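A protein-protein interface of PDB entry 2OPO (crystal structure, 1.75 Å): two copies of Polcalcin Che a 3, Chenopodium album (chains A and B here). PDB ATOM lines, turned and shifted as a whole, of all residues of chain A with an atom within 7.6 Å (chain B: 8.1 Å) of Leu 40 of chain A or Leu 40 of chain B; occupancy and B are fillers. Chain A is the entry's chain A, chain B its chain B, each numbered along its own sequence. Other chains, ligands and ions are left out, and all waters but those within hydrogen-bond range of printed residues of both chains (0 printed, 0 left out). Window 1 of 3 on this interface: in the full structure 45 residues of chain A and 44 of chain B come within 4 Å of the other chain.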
ATOM      1  N   PHE A  20     -20.665 -28.230 -33.045  1.00  0.00           N
ATOM      2  CA  PHE A  20     -21.379 -28.678 -31.841  1.00  0.00           C
ATOM      3  C   PHE A  20     -22.580 -29.525 -32.280  1.00  0.00           C
ATOM      4  O   PHE A  20     -22.943 -30.459 -31.588  1.00  0.00           O
ATOM      5  CB  PHE A  20     -21.888 -27.503 -31.030  1.00  0.00           C
ATOM      6  CG  PHE A  20     -20.886 -26.893 -30.118  1.00  0.00           C
ATOM      7  CD1 PHE A  20     -19.609 -26.563 -30.557  1.00  0.00           C
ATOM      8  CD2 PHE A  20     -21.227 -26.620 -28.801  1.00  0.00           C
ATOM      9  CE1 PHE A  20     -18.669 -25.970 -29.669  1.00  0.00           C
ATOM     10  CE2 PHE A  20     -20.293 -26.038 -27.918  1.00  0.00           C
ATOM     11  CZ  PHE A  20     -19.014 -25.710 -28.385  1.00  0.00           C
ATOM     12  N   GLY A  34     -22.891 -31.058 -24.046  1.00  0.00           N
ATOM     13  CA  GLY A  34     -21.988 -31.709 -23.113  1.00  0.00           C
ATOM     14  C   GLY A  34     -20.834 -32.390 -23.844  1.00  0.00           C
ATOM     15  O   GLY A  34     -19.681 -32.269 -23.426  1.00  0.00           O
ATOM     16  N   ASP A  35     -21.128 -33.043 -24.973  1.00  0.00           N
ATOM     17  CA  ASP A  35     -20.111 -33.701 -25.802  1.00  0.00           C
ATOM     18  C   ASP A  35     -19.102 -32.680 -26.309  1.00  0.00           C
ATOM     19  O   ASP A  35     -17.914 -32.925 -26.273  1.00  0.00           O
ATOM     20  CB  ASP A  35     -20.727 -34.389 -27.038  1.00  0.00           C
ATOM     21  CG  ASP A  35     -21.491 -35.634 -26.733  1.00  0.00           C
ATOM     22  OD1 ASP A  35     -21.403 -36.194 -25.626  1.00  0.00           O
ATOM     23  OD2 ASP A  35     -22.188 -36.076 -27.707  1.00  0.00           O
ATOM     24  N   ALA A  36     -19.558 -31.537 -26.745  1.00  0.00           N
ATOM     25  CA  ALA A  36     -18.659 -30.470 -27.244  1.00  0.00           C
ATOM     26  C   ALA A  36     -17.738 -29.971 -26.137  1.00  0.00           C
ATOM     27  O   ALA A  36     -16.503 -29.998 -26.284  1.00  0.00           O
ATOM     28  CB  ALA A  36     -19.441 -29.369 -27.774  1.00  0.00           C
ATOM     29  N   LEU A  37     -18.328 -29.607 -25.004  1.00  0.00           N
ATOM     30  CA  LEU A  37     -17.528 -29.105 -23.857  1.00  0.00           C
ATOM     31  C   LEU A  37     -16.454 -30.100 -23.507  1.00  0.00           C
ATOM     32  O   LEU A  37     -15.266 -29.728 -23.286  1.00  0.00           O
ATOM     33  CB  LEU A  37     -18.403 -28.779 -22.639  1.00  0.00           C
ATOM     34  CG  LEU A  37     -19.476 -27.673 -22.789  1.00  0.00           C
ATOM     35  CD1 LEU A  37     -20.395 -27.558 -21.569  1.00  0.00           C
ATOM     36  CD2 LEU A  37     -18.819 -26.346 -23.151  1.00  0.00           C
ATOM     37  N   LYS A  38     -16.855 -31.367 -23.413  1.00  0.00           N
ATOM     38  CA  LYS A  38     -15.956 -32.444 -23.024  1.00  0.00           C
ATOM     39  C   LYS A  38     -14.744 -32.577 -23.922  1.00  0.00           C
ATOM     40  O   LYS A  38     -13.686 -32.978 -23.451  1.00  0.00           O
ATOM     41  CB  LYS A  38     -16.677 -33.788 -22.919  1.00  0.00           C
ATOM     42  CG  LYS A  38     -17.321 -33.965 -21.522  1.00  0.00           C
ATOM     43  CD  LYS A  38     -18.215 -35.235 -21.314  1.00  0.00           C
ATOM     44  CE  LYS A  38     -18.962 -35.667 -22.561  1.00  0.00           C
ATOM     45  NZ  LYS A  38     -20.233 -36.553 -22.410  1.00  0.00           N
ATOM     46  N   THR A  39     -14.863 -32.263 -25.202  1.00  0.00           N
ATOM     47  CA  THR A  39     -13.682 -32.492 -26.053  1.00  0.00           C
ATOM     48  C   THR A  39     -12.492 -31.557 -25.678  1.00  0.00           C
ATOM     49  O   THR A  39     -11.458 -31.551 -26.328  1.00  0.00           O
ATOM     50  CB  THR A  39     -14.033 -32.435 -27.524  1.00  0.00           C
ATOM     51  OG1 THR A  39     -14.472 -31.115 -27.846  1.00  0.00           O
ATOM     52  CG2 THR A  39     -15.179 -33.456 -27.870  1.00  0.00           C
ATOM     53  N   LEU A  40     -12.603 -30.828 -24.568  1.00  0.00           N
ATOM     54  CA  LEU A  40     -11.508 -29.972 -24.114  1.00  0.00           C
ATOM     55  C   LEU A  40     -10.614 -30.638 -23.067  1.00  0.00           C
ATOM     56  O   LEU A  40      -9.463 -30.264 -22.877  1.00  0.00           O
ATOM     57  CB  LEU A  40     -12.066 -28.682 -23.611  1.00  0.00           C
ATOM     58  CG  LEU A  40     -12.983 -27.953 -24.590  1.00  0.00           C
ATOM     59  CD1 LEU A  40     -13.150 -26.506 -24.133  1.00  0.00           C
ATOM     60  CD2 LEU A  40     -12.510 -28.016 -26.025  1.00  0.00           C
ATOM     61  N   GLY A  41     -11.109 -31.657 -22.389  1.00  0.00           N
ATOM     62  CA  GLY A  41     -10.228 -32.463 -21.556  1.00  0.00           C
ATOM     63  C   GLY A  41      -9.018 -32.924 -22.369  1.00  0.00           C
ATOM     64  O   GLY A  41      -7.976 -33.262 -21.799  1.00  0.00           O
ATOM     65  N   SER A  42      -9.193 -32.966 -23.703  1.00  0.00           N
ATOM     66  CA  SER A  42      -8.149 -33.310 -24.674  1.00  0.00           C
ATOM     67  C   SER A  42      -7.905 -32.096 -25.575  1.00  0.00           C
ATOM     68  O   SER A  42      -8.045 -32.158 -26.811  1.00  0.00           O
ATOM     69  CB  SER A  42      -8.619 -34.493 -25.523  1.00  0.00           C
ATOM     70  OG  SER A  42      -9.863 -34.140 -26.108  1.00  0.00           O
ATOM     71  N   VAL A  43      -7.541 -30.979 -24.961  1.00  0.00           N
ATOM     72  CA  VAL A  43      -7.236 -29.809 -25.761  1.00  0.00           C
ATOM     73  C   VAL A  43      -5.789 -29.971 -26.194  1.00  0.00           C
ATOM     74  O   VAL A  43      -4.929 -30.207 -25.353  1.00  0.00           O
ATOM     75  CB  VAL A  43      -7.475 -28.466 -24.990  1.00  0.00           C
ATOM     76  CG1 VAL A  43      -6.611 -28.375 -23.756  1.00  0.00           C
ATOM     77  CG2 VAL A  43      -7.257 -27.317 -25.932  1.00  0.00           C
ATOM     78  N   THR A  44      -5.508 -29.859 -27.495  1.00  0.00           N
ATOM     79  CA  THR A  44      -4.154 -30.148 -27.975  1.00  0.00           C
ATOM     80  C   THR A  44      -3.177 -29.068 -27.574  1.00  0.00           C
ATOM     81  O   THR A  44      -3.558 -27.924 -27.299  1.00  0.00           O
ATOM     82  CB  THR A  44      -4.045 -30.363 -29.525  1.00  0.00           C
ATOM     83  OG1 THR A  44      -4.061 -29.093 -30.180  1.00  0.00           O
ATOM     84  CG2 THR A  44      -5.137 -31.285 -30.083  1.00  0.00           C
ATOM     85  N   GLU A  47      -3.429 -26.064 -29.884  1.00  0.00           N
ATOM     86  CA  GLU A  47      -4.682 -25.331 -29.624  1.00  0.00           C
ATOM     87  C   GLU A  47      -4.554 -24.427 -28.414  1.00  0.00           C
ATOM     88  O   GLU A  47      -5.040 -23.289 -28.431  1.00  0.00           O
ATOM     89  CB  GLU A  47      -5.887 -26.304 -29.503  1.00  0.00           C
ATOM     90  CG  GLU A  47      -6.290 -26.988 -30.804  1.00  0.00           C
ATOM     91  CD  GLU A  47      -7.211 -28.233 -30.599  1.00  0.00           C
ATOM     92  OE1 GLU A  47      -7.422 -28.654 -29.440  1.00  0.00           O
ATOM     93  OE2 GLU A  47      -7.738 -28.785 -31.594  1.00  0.00           O
ATOM     94  N   VAL A  48      -3.889 -24.896 -27.351  1.00  0.00           N
ATOM     95  CA  VAL A  48      -3.702 -24.081 -26.169  1.00  0.00           C
ATOM     96  C   VAL A  48      -2.832 -22.875 -26.493  1.00  0.00           C
ATOM     97  O   VAL A  48      -3.137 -21.755 -26.118  1.00  0.00           O
ATOM     98  CB  VAL A  48      -3.131 -24.888 -24.982  1.00  0.00           C
ATOM     99  CG1 VAL A  48      -2.849 -23.982 -23.862  1.00  0.00           C
ATOM    100  CG2 VAL A  48      -4.120 -26.029 -24.524  1.00  0.00           C
ATOM    101  N   MET A  51      -4.996 -20.216 -28.307  1.00  0.00           N
ATOM    102  CA  MET A  51      -5.865 -19.472 -27.417  1.00  0.00           C
ATOM    103  C   MET A  51      -5.064 -18.543 -26.537  1.00  0.00           C
ATOM    104  O   MET A  51      -5.444 -17.413 -26.311  1.00  0.00           O
ATOM    105  CB  MET A  51      -6.697 -20.391 -26.536  1.00  0.00           C
ATOM    106  CG  MET A  51      -7.747 -19.602 -25.751  1.00  0.00           C
ATOM    107  SD  MET A  51      -8.786 -20.734 -24.822  1.00  0.00           S
ATOM    108  CE  MET A  51      -9.161 -21.935 -26.105  1.00  0.00           C
ATOM    109  N   VAL A  82     -19.227 -18.790 -16.519  1.00  0.00           N
ATOM    110  CA  VAL A  82     -18.066 -19.591 -16.115  1.00  0.00           C
ATOM    111  C   VAL A  82     -17.811 -19.529 -14.621  1.00  0.00           C
ATOM    112  O   VAL A  82     -17.581 -20.560 -13.997  1.00  0.00           O
ATOM    113  CB  VAL A  82     -16.788 -19.144 -16.826  1.00  0.00           C
ATOM    114  CG1 VAL A  82     -15.559 -19.879 -16.256  1.00  0.00           C
ATOM    115  CG2 VAL A  82     -16.926 -19.371 -18.326  1.00  0.00           C
ATOM    116  N   PHE A  86     -19.115 -23.246 -13.378  1.00  0.00           N
ATOM    117  CA  PHE A  86     -17.930 -24.095 -13.374  1.00  0.00           C
ATOM    118  C   PHE A  86     -17.012 -23.789 -12.201  1.00  0.00           C
ATOM    119  O   PHE A  86     -17.424 -23.192 -11.196  1.00  0.00           O
ATOM    120  CB  PHE A  86     -17.178 -23.929 -14.692  1.00  0.00           C
ATOM    121  CG  PHE A  86     -17.991 -24.307 -15.875  1.00  0.00           C
ATOM    122  CD1 PHE A  86     -18.005 -25.603 -16.319  1.00  0.00           C
ATOM    123  CD2 PHE A  86     -18.780 -23.371 -16.512  1.00  0.00           C
ATOM    124  CE1 PHE A  86     -18.790 -25.973 -17.413  1.00  0.00           C
ATOM    125  CE2 PHE A  86     -19.558 -23.715 -17.603  1.00  0.00           C
ATOM    126  CZ  PHE A  86     -19.571 -25.032 -18.057  1.00  0.00           C
ATOM    127  OXT PHE A  86     -15.831 -24.157 -12.243  1.00  0.00           O
ATOM    128  N   LEU B  33      -3.539 -22.135 -18.391  1.00  0.00           N
ATOM    129  CA  LEU B  33      -4.689 -22.020 -19.311  1.00  0.00           C
ATOM    130  C   LEU B  33      -5.135 -23.381 -19.799  1.00  0.00           C
ATOM    131  O   LEU B  33      -6.324 -23.660 -19.742  1.00  0.00           O
ATOM    132  CB  LEU B  33      -4.398 -21.068 -20.448  1.00  0.00           C
ATOM    133  CG  LEU B  33      -5.429 -20.905 -21.515  1.00  0.00           C
ATOM    134  CD1 LEU B  33      -6.573 -20.187 -20.842  1.00  0.00           C
ATOM    135  CD2 LEU B  33      -4.927 -20.072 -22.656  1.00  0.00           C
ATOM    136  N   GLY B  34      -4.211 -24.231 -20.205  1.00  0.00           N
ATOM    137  CA  GLY B  34      -4.515 -25.569 -20.652  1.00  0.00           C
ATOM    138  C   GLY B  34      -5.199 -26.373 -19.546  1.00  0.00           C
ATOM    139  O   GLY B  34      -6.195 -27.057 -19.806  1.00  0.00           O
ATOM    140  N   ASP B  35      -4.721 -26.225 -18.306  1.00  0.00           N
ATOM    141  CA  ASP B  35      -5.325 -26.961 -17.157  1.00  0.00           C
ATOM    142  C   ASP B  35      -6.776 -26.526 -16.918  1.00  0.00           C
ATOM    143  O   ASP B  35      -7.645 -27.318 -16.643  1.00  0.00           O
ATOM    144  CB  ASP B  35      -4.504 -26.721 -15.881  1.00  0.00           C
ATOM    145  CG  ASP B  35      -3.204 -27.524 -15.839  1.00  0.00           C
ATOM    146  OD1 ASP B  35      -2.998 -28.378 -16.726  1.00  0.00           O
ATOM    147  OD2 ASP B  35      -2.392 -27.263 -14.910  1.00  0.00           O
ATOM    148  N   ALA B  36      -7.021 -25.247 -17.025  1.00  0.00           N
ATOM    149  CA  ALA B  36      -8.372 -24.688 -16.898  1.00  0.00           C
ATOM    150  C   ALA B  36      -9.289 -25.294 -17.979  1.00  0.00           C
ATOM    151  O   ALA B  36     -10.402 -25.753 -17.661  1.00  0.00           O
ATOM    152  CB  ALA B  36      -8.334 -23.192 -17.064  1.00  0.00           C
ATOM    153  N   LEU B  37      -8.818 -25.290 -19.244  1.00  0.00           N
ATOM    154  CA  LEU B  37      -9.618 -25.817 -20.357  1.00  0.00           C
ATOM    155  C   LEU B  37      -9.887 -27.312 -20.125  1.00  0.00           C
ATOM    156  O   LEU B  37     -10.978 -27.787 -20.420  1.00  0.00           O
ATOM    157  CB  LEU B  37      -8.931 -25.583 -21.689  1.00  0.00           C
ATOM    158  CG  LEU B  37      -8.884 -24.164 -22.253  1.00  0.00           C
ATOM    159  CD1 LEU B  37      -7.903 -24.069 -23.405  1.00  0.00           C
ATOM    160  CD2 LEU B  37     -10.262 -23.689 -22.735  1.00  0.00           C
ATOM    161  N   LYS B  38      -8.889 -28.044 -19.612  1.00  0.00           N
ATOM    162  CA  LYS B  38      -8.972 -29.470 -19.333  1.00  0.00           C
ATOM    163  C   LYS B  38     -10.003 -29.877 -18.287  1.00  0.00           C
ATOM    164  O   LYS B  38     -10.480 -31.035 -18.310  1.00  0.00           O
ATOM    165  CB  LYS B  38      -7.612 -30.018 -18.922  1.00  0.00           C
ATOM    166  CG  LYS B  38      -6.709 -30.140 -20.109  1.00  0.00           C
ATOM    167  CD  LYS B  38      -5.296 -30.346 -19.693  1.00  0.00           C
ATOM    168  CE  LYS B  38      -4.435 -30.404 -20.939  1.00  0.00           C
ATOM    169  NZ  LYS B  38      -3.014 -30.672 -20.531  1.00  0.00           N
ATOM    170  N   THR B  39     -10.384 -28.951 -17.411  1.00  0.00           N
ATOM    171  CA  THR B  39     -11.431 -29.260 -16.446  1.00  0.00           C
ATOM    172  C   THR B  39     -12.784 -29.463 -17.169  1.00  0.00           C
ATOM    173  O   THR B  39     -13.615 -30.162 -16.647  1.00  0.00           O
ATOM    174  CB  THR B  39     -11.647 -28.177 -15.377  1.00  0.00           C
ATOM    175  OG1 THR B  39     -12.158 -26.994 -15.984  1.00  0.00           O
ATOM    176  CG2 THR B  39     -10.321 -27.828 -14.609  1.00  0.00           C
ATOM    177  N   LEU B  40     -12.973 -28.906 -18.359  1.00  0.00           N
ATOM    178  CA  LEU B  40     -14.237 -29.160 -19.113  1.00  0.00           C
ATOM    179  C   LEU B  40     -14.448 -30.632 -19.527  1.00  0.00           C
ATOM    180  O   LEU B  40     -15.556 -31.074 -19.795  1.00  0.00           O
ATOM    181  CB  LEU B  40     -14.287 -28.280 -20.331  1.00  0.00           C
ATOM    182  CG  LEU B  40     -14.411 -26.789 -20.038  1.00  0.00           C
ATOM    183  CD1 LEU B  40     -14.250 -25.938 -21.324  1.00  0.00           C
ATOM    184  CD2 LEU B  40     -15.758 -26.491 -19.382  1.00  0.00           C
ATOM    185  N   GLY B  41     -13.384 -31.398 -19.610  1.00  0.00           N
ATOM    186  CA  GLY B  41     -13.463 -32.848 -19.810  1.00  0.00           C
ATOM    187  C   GLY B  41     -14.276 -33.617 -18.764  1.00  0.00           C
ATOM    188  O   GLY B  41     -14.700 -34.733 -19.010  1.00  0.00           O
ATOM    189  N   SER B  42     -14.418 -33.020 -17.581  1.00  0.00           N
ATOM    190  CA  SER B  42     -15.238 -33.568 -16.534  1.00  0.00           C
ATOM    191  C   SER B  42     -16.413 -32.695 -16.219  1.00  0.00           C
ATOM    192  O   SER B  42     -16.938 -32.736 -15.095  1.00  0.00           O
ATOM    193  CB  SER B  42     -14.447 -33.808 -15.267  1.00  0.00           C
ATOM    194  OG  SER B  42     -14.010 -32.588 -14.685  1.00  0.00           O
ATOM    195  N   VAL B  43     -16.927 -31.990 -17.228  1.00  0.00           N
ATOM    196  CA  VAL B  43     -18.092 -31.195 -16.963  1.00  0.00           C
ATOM    197  C   VAL B  43     -19.228 -32.125 -16.464  1.00  0.00           C
ATOM    198  O   VAL B  43     -19.404 -33.230 -16.964  1.00  0.00           O
ATOM    199  CB  VAL B  43     -18.511 -30.362 -18.181  1.00  0.00           C
ATOM    200  CG1 VAL B  43     -18.994 -31.246 -19.276  1.00  0.00           C
ATOM    201  CG2 VAL B  43     -19.559 -29.389 -17.743  1.00  0.00           C
ATOM    202  N   THR B  44     -19.995 -31.664 -15.479  1.00  0.00           N
ATOM    203  CA  THR B  44     -21.064 -32.520 -14.903  1.00  0.00           C
ATOM    204  C   THR B  44     -22.404 -32.339 -15.595  1.00  0.00           C
ATOM    205  O   THR B  44     -22.672 -31.253 -16.145  1.00  0.00           O
ATOM    206  CB  THR B  44     -21.294 -32.216 -13.410  1.00  0.00           C
ATOM    207  OG1 THR B  44     -21.827 -30.886 -13.302  1.00  0.00           O
ATOM    208  CG2 THR B  44     -19.998 -32.373 -12.615  1.00  0.00           C
ATOM    209  N   GLU B  47     -23.849 -29.128 -14.523  1.00  0.00           N
ATOM    210  CA  GLU B  47     -23.239 -27.966 -15.173  1.00  0.00           C
ATOM    211  C   GLU B  47     -23.720 -27.772 -16.611  1.00  0.00           C
ATOM    212  O   GLU B  47     -24.020 -26.644 -17.056  1.00  0.00           O
ATOM    213  CB  GLU B  47     -21.706 -28.074 -15.172  1.00  0.00           C
ATOM    214  CG  GLU B  47     -21.128 -27.758 -13.803  1.00  0.00           C
ATOM    215  CD  GLU B  47     -19.691 -28.201 -13.636  1.00  0.00           C
ATOM    216  OE1 GLU B  47     -19.195 -29.051 -14.418  1.00  0.00           O
ATOM    217  OE2 GLU B  47     -19.062 -27.721 -12.654  1.00  0.00           O
ATOM    218  N   VAL B  48     -23.828 -28.876 -17.320  1.00  0.00           N
ATOM    219  CA  VAL B  48     -24.374 -28.790 -18.667  1.00  0.00           C
ATOM    220  C   VAL B  48     -25.786 -28.235 -18.603  1.00  0.00           C
ATOM    221  O   VAL B  48     -26.110 -27.351 -19.352  1.00  0.00           O
ATOM    222  CB  VAL B  48     -24.381 -30.129 -19.395  1.00  0.00           C
ATOM    223  CG1 VAL B  48     -25.079 -29.944 -20.765  1.00  0.00           C
ATOM    224  CG2 VAL B  48     -22.963 -30.634 -19.601  1.00  0.00           C
ATOM    225  N   MET B  51     -25.779 -24.567 -18.112  1.00  0.00           N
ATOM    226  CA  MET B  51     -25.376 -23.809 -19.297  1.00  0.00           C
ATOM    227  C   MET B  51     -26.480 -23.847 -20.333  1.00  0.00           C
ATOM    228  O   MET B  51     -26.745 -22.858 -20.983  1.00  0.00           O
ATOM    229  CB  MET B  51     -24.043 -24.273 -19.881  1.00  0.00           C
ATOM    230  CG  MET B  51     -23.736 -23.578 -21.202  1.00  0.00           C
ATOM    231  SD  MET B  51     -22.061 -23.853 -21.754  1.00  0.00           S
ATOM    232  CE  MET B  51     -21.317 -22.370 -21.062  1.00  0.00           C
ATOM    233  N   VAL B  82     -12.733 -19.771 -29.467  1.00  0.00           N
ATOM    234  CA  VAL B  82     -13.261 -21.132 -29.470  1.00  0.00           C
ATOM    235  C   VAL B  82     -13.293 -21.699 -30.883  1.00  0.00           C
ATOM    236  O   VAL B  82     -12.945 -22.853 -31.099  1.00  0.00           O
ATOM    237  CB  VAL B  82     -14.677 -21.168 -28.819  1.00  0.00           C
ATOM    238  CG1 VAL B  82     -15.462 -22.428 -29.205  1.00  0.00           C
ATOM    239  CG2 VAL B  82     -14.547 -21.059 -27.329  1.00  0.00           C
ATOM    240  N   ILE B  85     -10.413 -24.085 -32.019  1.00  0.00           N
ATOM    241  CA  ILE B  85     -10.390 -25.428 -31.446  1.00  0.00           C
ATOM    242  C   ILE B  85     -11.453 -26.302 -32.124  1.00  0.00           C
ATOM    243  O   ILE B  85     -11.246 -27.491 -32.330  1.00  0.00           O
ATOM    244  CB  ILE B  85     -10.683 -25.379 -29.949  1.00  0.00           C
ATOM    245  CG1 ILE B  85      -9.654 -24.496 -29.243  1.00  0.00           C
ATOM    246  CG2 ILE B  85     -10.715 -26.783 -29.365  1.00  0.00           C
ATOM    247  CD1 ILE B  85      -9.759 -24.562 -27.742  1.00  0.00           C
ATOM    248  N   PHE B  86     -12.586 -25.692 -32.464  1.00  0.00           N
ATOM    249  CA  PHE B  86     -13.707 -26.373 -33.101  1.00  0.00           C
ATOM    250  C   PHE B  86     -13.809 -25.939 -34.555  1.00  0.00           C
ATOM    251  O   PHE B  86     -12.906 -26.188 -35.353  1.00  0.00           O
ATOM    252  CB  PHE B  86     -15.006 -26.018 -32.372  1.00  0.00           C
ATOM    253  CG  PHE B  86     -15.101 -26.586 -30.996  1.00  0.00           C
ATOM    254  CD1 PHE B  86     -15.279 -27.945 -30.797  1.00  0.00           C
ATOM    255  CD2 PHE B  86     -15.018 -25.761 -29.886  1.00  0.00           C
ATOM    256  CE1 PHE B  86     -15.368 -28.471 -29.507  1.00  0.00           C
ATOM    257  CE2 PHE B  86     -15.104 -26.284 -28.585  1.00  0.00           C
ATOM    258  CZ  PHE B  86     -15.282 -27.633 -28.401  1.00  0.00           C
ATOM    259  OXT PHE B  86     -14.799 -25.323 -34.963  1.00  0.00           O
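Of the printed residues of chain B, Gly 34 of chain A touches Val 48. Asp 35 of chain A touches none of the printed residues of chain B. Of the printed residues of chain B, Leu 37 of chain A touches Leu 40 (3.4 Å). Of the printed residues of chain B, Leu 40 of chain A touches Leu 37, Lys 38, Leu 40, Ile 85 and Phe 86. Thr 44 of chain A touches none of the printed residues of chain B. Of the printed residues of chain A, Lys 38 of chain B touches Leu 40 and Gly 41. Leu 40 of chain B touches four residues of chain A. Printed residues of chain A within 4 Å of Gly 41 of chain B: Lys 38 and Gly 41. The nearest printed residue of chain B that does not touch Leu 40 of chain A is Gly 41 of chain B (4.5 Å).
Lys 38 of chain A touches Leu 40 of chain B, and with the chains exchanged Leu 40 of chain A touches Lys 38 of chain B. Lys 38 of chain A touches Val 43 of chain B, but with the chains exchanged Val 43 of chain A does not touch Lys 38 of chain B (4.1 Å). Thr 39 of chain A touches Phe 86 of chain B, but with the chains exchanged Phe 86 of chain A does not touch Thr 39 of chain B (6.0 Å). Met 51 of chain A touches Leu 37 of chain B, but with the chains exchanged Leu 37 of chain A does not touch Met 51 of chain B (4.1 Å). Of the 22 pairs that touch across the chains among the printed residues, 12 have their exchanged pair printed and touching as well.
OD1 of Asp 35 of chain A is in salt-bridge range of NZ of Lys 38 of chain A (3.4 Å). The backbone carbonyl oxygen of Ala 36 of chain A is in hydrogen-bond range of the side-chain hydroxyl of Thr 39 of chain A (2.8 Å). The backbone carbonyl oxygen (O) of Thr 39 of chain A is in hydrogen-bond range of the side-chain hydroxyl (OG) of Ser 42 of chain A, 3.0 Å away. N of Thr 44 of chain A is in hydrogen-bond range of OE1 of Glu 47 of chain A (3.0 Å). The backbone NH (N) of Thr 44 of chain B sits at hydrogen-bond distance from the side-chain carboxylate (OE1) of Glu 47 of chain B (2.9 Å).
Phe 86 of chain B touches Phe 20 of chain A. Phe 86 of chain B touches Ala 36 of chain A (CZ to O, 3.4 Å). Leu 40 of chain B touches Leu 37 of chain A. CA of Lys 38 of chain A touches O of Leu 40 of chain B (3.5 Å). Lys 38 of chain A touches Gly 41 of chain B. CE1 of Phe 86 of chain B touches OG1 of Thr 39 of chain A, 3.2 Å away. Ile 85 of chain B touches Leu 40 of chain A (CG2 to CD2, 3.99 Å). Lys 38 of chain B touches Gly 41 of chain A (O to CA, 3.6 Å). Ile 85 of chain B touches Glu 47 of chain A (CG2 to OE1, 3.8 Å). Phe 86 of chain A touches Leu 40 of chain B (CE1 to CD2, 3.7 Å).
Of the 17 printed residues of chain A, 12 touch a printed residue of chain B. Hydrophobic or aromatic side chains of chain A that line the printed part of chain B: Phe 20, Leu 40, Val 48, Met 51 and Phe 86. Printed residues of chain B that touch a printed residue of chain A: Gly 34, Leu 37, Lys 38, Leu 40, Gly 41, Val 43, Glu 47, Val 48, Ile 85 and Phe 86. Hydrophobic or aromatic side chains of chain B within 4 Å of the printed part of chain A: Leu 37, Leu 40, Val 43, Val 48, Ile 85 and Phe 86.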
